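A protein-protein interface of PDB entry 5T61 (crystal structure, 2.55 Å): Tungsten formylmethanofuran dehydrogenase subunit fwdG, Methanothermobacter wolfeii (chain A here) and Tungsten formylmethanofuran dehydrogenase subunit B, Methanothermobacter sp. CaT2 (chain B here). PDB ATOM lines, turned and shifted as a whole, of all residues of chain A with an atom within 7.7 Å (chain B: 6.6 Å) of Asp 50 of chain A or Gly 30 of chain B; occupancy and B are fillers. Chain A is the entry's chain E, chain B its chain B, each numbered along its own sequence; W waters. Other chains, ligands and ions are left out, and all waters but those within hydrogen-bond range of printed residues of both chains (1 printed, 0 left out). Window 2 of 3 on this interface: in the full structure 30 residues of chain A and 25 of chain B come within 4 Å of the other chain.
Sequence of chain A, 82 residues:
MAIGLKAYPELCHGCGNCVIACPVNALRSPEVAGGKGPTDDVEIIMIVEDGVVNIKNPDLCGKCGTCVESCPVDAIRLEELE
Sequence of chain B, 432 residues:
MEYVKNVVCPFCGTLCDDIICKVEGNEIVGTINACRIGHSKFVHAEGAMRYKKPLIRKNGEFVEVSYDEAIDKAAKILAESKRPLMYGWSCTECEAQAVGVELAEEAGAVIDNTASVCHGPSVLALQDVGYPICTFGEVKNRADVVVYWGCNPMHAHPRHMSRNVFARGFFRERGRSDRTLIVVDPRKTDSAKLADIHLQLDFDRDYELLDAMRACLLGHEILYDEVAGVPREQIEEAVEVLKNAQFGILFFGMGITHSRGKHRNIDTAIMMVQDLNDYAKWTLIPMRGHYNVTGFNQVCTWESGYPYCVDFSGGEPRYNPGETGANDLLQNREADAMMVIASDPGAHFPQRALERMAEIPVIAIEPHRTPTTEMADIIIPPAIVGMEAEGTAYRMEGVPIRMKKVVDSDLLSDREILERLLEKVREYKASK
NZ of Lys 22 of chain B is in salt-bridge range of OE1 of Glu 49 of chain A.
The side-chain amino group (NZ) of Lys 22 of chain B is in salt-bridge range of the side-chain carboxylate (OD2) of Asp 50 of chain A (2.8 Å).
The backbone carbonyl oxygen of Thr 31 of chain B lies within hydrogen-bond range of the backbone NH of Asp 50 of chain A (2.7 Å).
N of Asn 33 of chain B lies within hydrogen-bond range of O of Val 48 of chain A (2.8 Å).
NE of Arg 36 of chain B lies within hydrogen-bond range of O of Cys 12 of chain A (2.7 Å).
O of Gly 51 of chain A sits at hydrogen-bond distance from N of Arg 36 of chain B, at 3.3 Å.
O of Ile 20 of chain B sits at hydrogen-bond distance from N of Ile 32 of chain B, at 2.9 Å.
The backbone NH (N) of Val 29 of chain B is in hydrogen-bond range of the backbone carbonyl oxygen (O) of Lys 22 of chain B, at 2.9 Å.
O of Gly 30 of chain B is in hydrogen-bond range of N of Lys 22 of chain B, at 2.8 Å.
N of Gly 14 of chain A sits close to O of Gly 51 of chain A (3.4 Å).
O of Ile 47 of chain A lies within hydrogen-bond range of N of Asn 54 of chain A, at 2.8 Å.
The side-chain amino group of Lys 56 of chain A is in salt-bridge range of the side-chain carboxylate of Glu 49 of chain A, at 2.8 Å.
Among the printed residues, merely in contact across the chains: Gly 14 of chain A with Cys 35 of chain B, Ile 47 of chain A with Asn 33 of chain B, Val 48 of chain A with Ile 32 of chain B, Val 48 of chain A with Ala 34 of chain B, Glu 49 of chain A with Thr 31 of chain B, Asp 50 of chain A with Gly 30 of chain B, Asp 50 of chain A with His 39 of chain B, Gly 51 of chain A with Ala 34 of chain B, Gly 51 of chain A with Cys 35 of chain B, Gly 51 of chain A with His 39 of chain B and Val 52 of chain A with Arg 36 of chain B.
Printed residues of chain B within 4 Å of Asp 50 of chain A: Lys 22 (2.8 Å), Gly 30 (3.0 Å), Thr 31 (2.7 Å) and His 39 (3.3 Å).
Gly 30 of chain B touches just one residue of chain A: Asp 50 (3.0 Å).
Of the printed residues of chain B, Val 48 of chain A touches Ile 32 (3.5 Å), Asn 33 (2.8 Å) and Ala 34 (3.1 Å).
Printed residues of chain B within 4 Å of Gly 51 of chain A: Ala 34 (3.5 Å), Cys 35 (3.7 Å), Arg 36 (3.3 Å) and His 39 (3.8 Å).
Of the printed residues of chain B, Val 52 of chain A touches Arg 36.
Asn 54 of chain A touches none of the printed residues of chain B.
Glu 27 of chain B touches none of the printed residues of chain A.
The nearest residue of chain B that does not touch Asp 50 of chain A is Val 29 of chain B (4.1 Å).
The nearest residue of chain A that does not touch Gly 30 of chain B is Glu 49 of chain A (6.9 Å).
Hydrophobic or aromatic side chains of chain A within 4 Å of the printed part of chain B: Ile 47, Val 48 and Val 52.
Of the 18 printed residues of chain B, 9 touch a printed residue of chain A.
Hydrophobic or aromatic side chains of chain B that line the printed part of chain A: Ile 32 and His 39.
Among the printed residues, 17 pairs touch across the chains.
Among the printed residues, Asp or Glu carboxylates within 4 Å of a Lys or Arg side-chain nitrogen of the other chain: Glu 49 of chain A with Lys 22 of chain B and Asp 50 of chain A with Lys 22 of chain B.
Water W1 bridges O of Gly 14 of chain A (2.7 Å) and O of Asn 33 of chain B (2.7 Å).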
ATOM      1  N   CYS A  12     -20.878 -32.244 -10.284  1.00  0.00           N
ATOM      2  CA  CYS A  12     -21.413 -31.569 -11.456  1.00  0.00           C
ATOM      3  C   CYS A  12     -20.392 -30.658 -12.131  1.00  0.00           C
ATOM      4  O   CYS A  12     -19.558 -30.027 -11.476  1.00  0.00           O
ATOM      5  CB  CYS A  12     -22.629 -30.742 -11.051  1.00  0.00           C
ATOM      6  SG  CYS A  12     -23.052 -29.503 -12.260  1.00  0.00           S
ATOM      7  N   GLY A  14     -21.641 -28.264 -14.445  1.00  0.00           N
ATOM      8  CA  GLY A  14     -22.357 -27.123 -14.973  1.00  0.00           C
ATOM      9  C   GLY A  14     -22.538 -27.144 -16.474  1.00  0.00           C
ATOM     10  O   GLY A  14     -22.800 -26.096 -17.071  1.00  0.00           O
ATOM     11  N   ILE A  47     -31.892 -25.761 -13.275  1.00  0.00           N
ATOM     12  CA  ILE A  47     -31.000 -24.906 -14.046  1.00  0.00           C
ATOM     13  C   ILE A  47     -29.597 -25.073 -13.478  1.00  0.00           C
ATOM     14  O   ILE A  47     -29.400 -25.595 -12.376  1.00  0.00           O
ATOM     15  CB  ILE A  47     -31.411 -23.408 -14.025  1.00  0.00           C
ATOM     16  CG1 ILE A  47     -32.934 -23.241 -14.023  1.00  0.00           C
ATOM     17  CG2 ILE A  47     -30.808 -22.654 -15.215  1.00  0.00           C
ATOM     18  CD1 ILE A  47     -33.401 -21.865 -13.591  1.00  0.00           C
ATOM     19  N   VAL A  48     -28.619 -24.588 -14.233  1.00  0.00           N
ATOM     20  CA  VAL A  48     -27.260 -24.445 -13.731  1.00  0.00           C
ATOM     21  C   VAL A  48     -27.175 -23.103 -13.020  1.00  0.00           C
ATOM     22  O   VAL A  48     -27.461 -22.053 -13.607  1.00  0.00           O
ATOM     23  CB  VAL A  48     -26.235 -24.536 -14.869  1.00  0.00           C
ATOM     24  CG1 VAL A  48     -24.846 -24.259 -14.342  1.00  0.00           C
ATOM     25  CG2 VAL A  48     -26.293 -25.906 -15.528  1.00  0.00           C
ATOM     26  N   GLU A  49     -26.817 -23.137 -11.742  1.00  0.00           N
ATOM     27  CA  GLU A  49     -26.741 -21.923 -10.947  1.00  0.00           C
ATOM     28  C   GLU A  49     -25.485 -21.994 -10.100  1.00  0.00           C
ATOM     29  O   GLU A  49     -25.219 -23.023  -9.470  1.00  0.00           O
ATOM     30  CB  GLU A  49     -27.978 -21.766 -10.055  1.00  0.00           C
ATOM     31  CG  GLU A  49     -27.858 -20.661  -9.023  1.00  0.00           C
ATOM     32  CD  GLU A  49     -29.199 -20.221  -8.478  1.00  0.00           C
ATOM     33  OE1 GLU A  49     -29.335 -19.038  -8.107  1.00  0.00           O
ATOM     34  OE2 GLU A  49     -30.110 -21.067  -8.393  1.00  0.00           O
ATOM     35  N   ASP A  50     -24.731 -20.896 -10.077  1.00  0.00           N
ATOM     36  CA  ASP A  50     -23.404 -20.865  -9.464  1.00  0.00           C
ATOM     37  C   ASP A  50     -22.561 -22.077  -9.864  1.00  0.00           C
ATOM     38  O   ASP A  50     -21.887 -22.697  -9.038  1.00  0.00           O
ATOM     39  CB  ASP A  50     -23.516 -20.731  -7.944  1.00  0.00           C
ATOM     40  CG  ASP A  50     -24.333 -19.519  -7.528  1.00  0.00           C
ATOM     41  OD1 ASP A  50     -23.765 -18.410  -7.490  1.00  0.00           O
ATOM     42  OD2 ASP A  50     -25.539 -19.668  -7.245  1.00  0.00           O
ATOM     43  N   GLY A  51     -22.603 -22.419 -11.151  1.00  0.00           N
ATOM     44  CA  GLY A  51     -21.708 -23.394 -11.740  1.00  0.00           C
ATOM     45  C   GLY A  51     -22.136 -24.846 -11.673  1.00  0.00           C
ATOM     46  O   GLY A  51     -21.401 -25.704 -12.179  1.00  0.00           O
ATOM     47  N   VAL A  52     -23.285 -25.163 -11.064  1.00  0.00           N
ATOM     48  CA  VAL A  52     -23.712 -26.546 -10.873  1.00  0.00           C
ATOM     49  C   VAL A  52     -25.228 -26.673 -11.038  1.00  0.00           C
ATOM     50  O   VAL A  52     -25.966 -25.686 -11.026  1.00  0.00           O
ATOM     51  CB  VAL A  52     -23.294 -27.133  -9.501  1.00  0.00           C
ATOM     52  CG1 VAL A  52     -21.779 -27.227  -9.390  1.00  0.00           C
ATOM     53  CG2 VAL A  52     -23.868 -26.313  -8.357  1.00  0.00           C
ATOM     54  N   VAL A  53     -25.680 -27.922 -11.188  1.00  0.00           N
ATOM     55  CA  VAL A  53     -27.097 -28.211 -11.346  1.00  0.00           C
ATOM     56  C   VAL A  53     -27.841 -27.857 -10.075  1.00  0.00           C
ATOM     57  O   VAL A  53     -27.343 -28.048  -8.960  1.00  0.00           O
ATOM     58  CB  VAL A  53     -27.325 -29.689 -11.672  1.00  0.00           C
ATOM     59  CG1 VAL A  53     -28.743 -29.927 -12.184  1.00  0.00           C
ATOM     60  CG2 VAL A  53     -26.374 -30.066 -12.659  1.00  0.00           C
ATOM     61  N   ASN A  54     -29.048 -27.322 -10.245  1.00  0.00           N
ATOM     62  CA  ASN A  54     -29.806 -26.826  -9.110  1.00  0.00           C
ATOM     63  C   ASN A  54     -31.280 -27.082  -9.384  1.00  0.00           C
ATOM     64  O   ASN A  54     -31.851 -26.485 -10.302  1.00  0.00           O
ATOM     65  CB  ASN A  54     -29.524 -25.341  -8.900  1.00  0.00           C
ATOM     66  CG  ASN A  54     -30.145 -24.818  -7.643  1.00  0.00           C
ATOM     67  OD1 ASN A  54     -31.338 -24.982  -7.399  1.00  0.00           O
ATOM     68  ND2 ASN A  54     -29.329 -24.167  -6.829  1.00  0.00           N
ATOM     69  N   LYS A  56     -35.096 -26.752  -9.077  1.00  0.00           N
ATOM     70  CA  LYS A  56     -36.009 -25.675  -8.712  1.00  0.00           C
ATOM     71  C   LYS A  56     -37.471 -26.086  -8.613  1.00  0.00           C
ATOM     72  O   LYS A  56     -38.192 -25.536  -7.781  1.00  0.00           O
ATOM     73  CB  LYS A  56     -35.911 -24.532  -9.730  1.00  0.00           C
ATOM     74  CG  LYS A  56     -34.545 -23.901  -9.837  1.00  0.00           C
ATOM     75  CD  LYS A  56     -34.228 -23.172  -8.550  1.00  0.00           C
ATOM     76  CE  LYS A  56     -32.983 -22.327  -8.681  1.00  0.00           C
ATOM     77  NZ  LYS A  56     -32.581 -21.783  -7.357  1.00  0.00           N
ATOM     78  N   MET B   1     -29.983  -7.278  -4.073  1.00  0.00           N
ATOM     79  CA  MET B   1     -29.360  -8.057  -5.138  1.00  0.00           C
ATOM     80  C   MET B   1     -29.850  -7.645  -6.505  1.00  0.00           C
ATOM     81  O   MET B   1     -31.035  -7.388  -6.660  1.00  0.00           O
ATOM     82  CB  MET B   1     -29.632  -9.550  -4.933  1.00  0.00           C
ATOM     83  CG  MET B   1     -29.202 -10.405  -6.109  1.00  0.00           C
ATOM     84  SD  MET B   1     -27.505 -10.978  -5.949  1.00  0.00           S
ATOM     85  CE  MET B   1     -27.757 -12.457  -4.985  1.00  0.00           C
ATOM     86  N   ILE B  20     -26.015 -14.931 -16.658  1.00  0.00           N
ATOM     87  CA  ILE B  20     -26.593 -14.007 -15.695  1.00  0.00           C
ATOM     88  C   ILE B  20     -25.592 -13.843 -14.560  1.00  0.00           C
ATOM     89  O   ILE B  20     -25.105 -14.836 -14.003  1.00  0.00           O
ATOM     90  CB  ILE B  20     -27.945 -14.526 -15.189  1.00  0.00           C
ATOM     91  CG1 ILE B  20     -28.812 -14.949 -16.382  1.00  0.00           C
ATOM     92  CG2 ILE B  20     -28.636 -13.464 -14.341  1.00  0.00           C
ATOM     93  CD1 ILE B  20     -30.237 -14.478 -16.342  1.00  0.00           C
ATOM     94  N   CYS B  21     -25.251 -12.600 -14.245  1.00  0.00           N
ATOM     95  CA  CYS B  21     -24.374 -12.296 -13.125  1.00  0.00           C
ATOM     96  C   CYS B  21     -25.205 -11.826 -11.941  1.00  0.00           C
ATOM     97  O   CYS B  21     -26.097 -10.984 -12.094  1.00  0.00           O
ATOM     98  CB  CYS B  21     -23.346 -11.225 -13.499  1.00  0.00           C
ATOM     99  SG  CYS B  21     -21.984 -11.788 -14.540  1.00  0.00           S
ATOM    100  N   LYS B  22     -24.912 -12.372 -10.766  1.00  0.00           N
ATOM    101  CA  LYS B  22     -25.507 -11.883  -9.531  1.00  0.00           C
ATOM    102  C   LYS B  22     -24.555 -10.865  -8.925  1.00  0.00           C
ATOM    103  O   LYS B  22     -23.430 -11.207  -8.544  1.00  0.00           O
ATOM    104  CB  LYS B  22     -25.782 -13.010  -8.534  1.00  0.00           C
ATOM    105  CG  LYS B  22     -26.697 -14.107  -9.027  1.00  0.00           C
ATOM    106  CD  LYS B  22     -26.888 -15.134  -7.920  1.00  0.00           C
ATOM    107  CE  LYS B  22     -27.585 -16.383  -8.419  1.00  0.00           C
ATOM    108  NZ  LYS B  22     -27.365 -17.524  -7.485  1.00  0.00           N
ATOM    109  N   VAL B  23     -25.016  -9.624  -8.819  1.00  0.00           N
ATOM    110  CA  VAL B  23     -24.214  -8.509  -8.338  1.00  0.00           C
ATOM    111  C   VAL B  23     -24.854  -8.026  -7.049  1.00  0.00           C
ATOM    112  O   VAL B  23     -26.062  -7.765  -7.013  1.00  0.00           O
ATOM    113  CB  VAL B  23     -24.132  -7.379  -9.382  1.00  0.00           C
ATOM    114  CG1 VAL B  23     -23.176  -6.292  -8.924  1.00  0.00           C
ATOM    115  CG2 VAL B  23     -23.719  -7.942 -10.736  1.00  0.00           C
ATOM    116  N   GLU B  27     -20.026  -6.130  -6.313  1.00  0.00           N
ATOM    117  CA  GLU B  27     -19.152  -7.274  -6.483  1.00  0.00           C
ATOM    118  C   GLU B  27     -20.008  -8.433  -6.978  1.00  0.00           C
ATOM    119  O   GLU B  27     -21.219  -8.473  -6.744  1.00  0.00           O
ATOM    120  CB  GLU B  27     -18.213  -7.574  -5.247  1.00  0.00           C
ATOM    121  CG  GLU B  27     -18.750  -7.952  -3.801  1.00  0.00           C
ATOM    122  CD  GLU B  27     -18.622  -9.320  -3.137  1.00  0.00           C
ATOM    123  OE1 GLU B  27     -19.248  -9.785  -2.231  1.00  0.00           O
ATOM    124  OE2 GLU B  27     -17.619  -9.882  -3.474  1.00  0.00           O
ATOM    125  N   ILE B  28     -19.391  -9.267  -7.813  1.00  0.00           N
ATOM    126  CA  ILE B  28     -20.056 -10.401  -8.444  1.00  0.00           C
ATOM    127  C   ILE B  28     -19.985 -11.589  -7.497  1.00  0.00           C
ATOM    128  O   ILE B  28     -18.914 -12.141  -7.242  1.00  0.00           O
ATOM    129  CB  ILE B  28     -19.420 -10.732  -9.803  1.00  0.00           C
ATOM    130  CG1 ILE B  28     -19.423  -9.506 -10.725  1.00  0.00           C
ATOM    131  CG2 ILE B  28     -20.101 -11.932 -10.460  1.00  0.00           C
ATOM    132  CD1 ILE B  28     -18.554  -9.660 -11.960  1.00  0.00           C
ATOM    133  N   VAL B  29     -21.147 -11.997  -6.995  1.00  0.00           N
ATOM    134  CA  VAL B  29     -21.235 -13.001  -5.943  1.00  0.00           C
ATOM    135  C   VAL B  29     -21.810 -14.318  -6.431  1.00  0.00           C
ATOM    136  O   VAL B  29     -21.772 -15.306  -5.679  1.00  0.00           O
ATOM    137  CB  VAL B  29     -22.056 -12.473  -4.750  1.00  0.00           C
ATOM    138  CG1 VAL B  29     -21.382 -11.244  -4.169  1.00  0.00           C
ATOM    139  CG2 VAL B  29     -23.459 -12.123  -5.210  1.00  0.00           C
ATOM    140  N   GLY B  30     -22.325 -14.375  -7.654  1.00  0.00           N
ATOM    141  CA  GLY B  30     -22.887 -15.607  -8.176  1.00  0.00           C
ATOM    142  C   GLY B  30     -23.205 -15.477  -9.648  1.00  0.00           C
ATOM    143  O   GLY B  30     -23.104 -14.397 -10.238  1.00  0.00           O
ATOM    144  N   THR B  31     -23.596 -16.608 -10.236  1.00  0.00           N
ATOM    145  CA  THR B  31     -23.901 -16.687 -11.656  1.00  0.00           C
ATOM    146  C   THR B  31     -25.081 -17.622 -11.874  1.00  0.00           C
ATOM    147  O   THR B  31     -25.439 -18.423 -11.007  1.00  0.00           O
ATOM    148  CB  THR B  31     -22.710 -17.199 -12.487  1.00  0.00           C
ATOM    149  OG1 THR B  31     -22.379 -18.533 -12.082  1.00  0.00           O
ATOM    150  CG2 THR B  31     -21.485 -16.306 -12.322  1.00  0.00           C
ATOM    151  N   ILE B  32     -25.695 -17.491 -13.048  1.00  0.00           N
ATOM    152  CA  ILE B  32     -26.654 -18.456 -13.568  1.00  0.00           C
ATOM    153  C   ILE B  32     -26.231 -18.820 -14.985  1.00  0.00           C
ATOM    154  O   ILE B  32     -25.703 -17.972 -15.714  1.00  0.00           O
ATOM    155  CB  ILE B  32     -28.100 -17.910 -13.538  1.00  0.00           C
ATOM    156  CG1 ILE B  32     -28.487 -17.493 -12.116  1.00  0.00           C
ATOM    157  CG2 ILE B  32     -29.089 -18.940 -14.073  1.00  0.00           C
ATOM    158  CD1 ILE B  32     -29.782 -16.707 -12.043  1.00  0.00           C
ATOM    159  N   ASN B  33     -26.416 -20.098 -15.348  1.00  0.00           N
ATOM    160  CA  ASN B  33     -26.176 -20.652 -16.683  1.00  0.00           C
ATOM    161  C   ASN B  33     -24.704 -20.917 -16.976  1.00  0.00           C
ATOM    162  O   ASN B  33     -24.384 -21.800 -17.778  1.00  0.00           O
ATOM    163  CB  ASN B  33     -26.760 -19.741 -17.769  1.00  0.00           C
ATOM    164  CG  ASN B  33     -28.258 -19.595 -17.657  1.00  0.00           C
ATOM    165  OD1 ASN B  33     -28.952 -20.515 -17.227  1.00  0.00           O
ATOM    166  ND2 ASN B  33     -28.765 -18.425 -18.023  1.00  0.00           N
ATOM    167  N   ALA B  34     -23.805 -20.146 -16.365  1.00  0.00           N
ATOM    168  CA  ALA B  34     -22.378 -20.388 -16.533  1.00  0.00           C
ATOM    169  C   ALA B  34     -21.995 -21.749 -15.966  1.00  0.00           C
ATOM    170  O   ALA B  34     -22.550 -22.209 -14.965  1.00  0.00           O
ATOM    171  CB  ALA B  34     -21.567 -19.286 -15.852  1.00  0.00           C
ATOM    172  N   CYS B  35     -21.034 -22.404 -16.615  1.00  0.00           N
ATOM    173  CA  CYS B  35     -20.613 -23.711 -16.139  1.00  0.00           C
ATOM    174  C   CYS B  35     -19.698 -23.545 -14.931  1.00  0.00           C
ATOM    175  O   CYS B  35     -19.439 -22.432 -14.463  1.00  0.00           O
ATOM    176  CB  CYS B  35     -19.887 -24.490 -17.228  1.00  0.00           C
ATOM    177  SG  CYS B  35     -18.115 -24.178 -17.200  1.00  0.00           S
ATOM    178  N   ARG B  36     -19.170 -24.670 -14.438  1.00  0.00           N
ATOM    179  CA  ARG B  36     -18.351 -24.637 -13.232  1.00  0.00           C
ATOM    180  C   ARG B  36     -17.123 -23.752 -13.411  1.00  0.00           C
ATOM    181  O   ARG B  36     -16.723 -23.040 -12.481  1.00  0.00           O
ATOM    182  CB  ARG B  36     -17.927 -26.050 -12.830  1.00  0.00           C
ATOM    183  CG  ARG B  36     -17.005 -26.065 -11.614  1.00  0.00           C
ATOM    184  CD  ARG B  36     -16.608 -27.463 -11.160  1.00  0.00           C
ATOM    185  NE  ARG B  36     -17.725 -28.247 -10.644  1.00  0.00           N
ATOM    186  CZ  ARG B  36     -18.125 -28.220  -9.379  1.00  0.00           C
ATOM    187  NH1 ARG B  36     -17.508 -27.435  -8.505  1.00  0.00           N
ATOM    188  NH2 ARG B  36     -19.142 -28.973  -8.985  1.00  0.00           N
ATOM    189  N   HIS B  39     -18.163 -19.869 -13.864  1.00  0.00           N
ATOM    190  CA  HIS B  39     -18.544 -19.376 -12.545  1.00  0.00           C
ATOM    191  C   HIS B  39     -17.320 -19.046 -11.696  1.00  0.00           C
ATOM    192  O   HIS B  39     -17.301 -18.026 -11.000  1.00  0.00           O
ATOM    193  CB  HIS B  39     -19.422 -20.406 -11.837  1.00  0.00           C
ATOM    194  CG  HIS B  39     -19.658 -20.103 -10.391  1.00  0.00           C
ATOM    195  ND1 HIS B  39     -20.587 -19.179  -9.968  1.00  0.00           N
ATOM    196  CD2 HIS B  39     -19.083 -20.602  -9.271  1.00  0.00           C
ATOM    197  CE1 HIS B  39     -20.578 -19.123  -8.647  1.00  0.00           C
ATOM    198  NE2 HIS B  39     -19.672 -19.976  -8.201  1.00  0.00           N
ATOM    199  N   PHE B  42     -15.927 -15.604 -12.573  1.00  0.00           N
ATOM    200  CA  PHE B  42     -16.759 -14.470 -12.180  1.00  0.00           C
ATOM    201  C   PHE B  42     -16.698 -14.210 -10.679  1.00  0.00           C
ATOM    202  O   PHE B  42     -16.787 -13.055 -10.249  1.00  0.00           O
ATOM    203  CB  PHE B  42     -18.211 -14.701 -12.607  1.00  0.00           C
ATOM    204  CG  PHE B  42     -18.482 -14.376 -14.046  1.00  0.00           C
ATOM    205  CD1 PHE B  42     -18.536 -13.063 -14.476  1.00  0.00           C
ATOM    206  CD2 PHE B  42     -18.711 -15.388 -14.966  1.00  0.00           C
ATOM    207  CE1 PHE B  42     -18.791 -12.763 -15.802  1.00  0.00           C
ATOM    208  CE2 PHE B  42     -18.970 -15.092 -16.292  1.00  0.00           C
ATOM    209  CZ  PHE B  42     -19.011 -13.778 -16.710  1.00  0.00           C
ATOM    210  N   VAL B  43     -16.567 -15.257  -9.871  1.00  0.00           N
ATOM    211  CA  VAL B  43     -16.639 -15.146  -8.419  1.00  0.00           C
ATOM    212  C   VAL B  43     -15.232 -15.194  -7.847  1.00  0.00           C
ATOM    213  O   VAL B  43     -14.375 -15.945  -8.334  1.00  0.00           O
ATOM    214  CB  VAL B  43     -17.510 -16.271  -7.829  1.00  0.00           C
ATOM    215  CG1 VAL B  43     -17.532 -16.205  -6.310  1.00  0.00           C
ATOM    216  CG2 VAL B  43     -18.920 -16.188  -8.384  1.00  0.00           C
HETATM  217  O   HOH W   1     -24.799 -24.495 -18.002  1.00  0.00           O
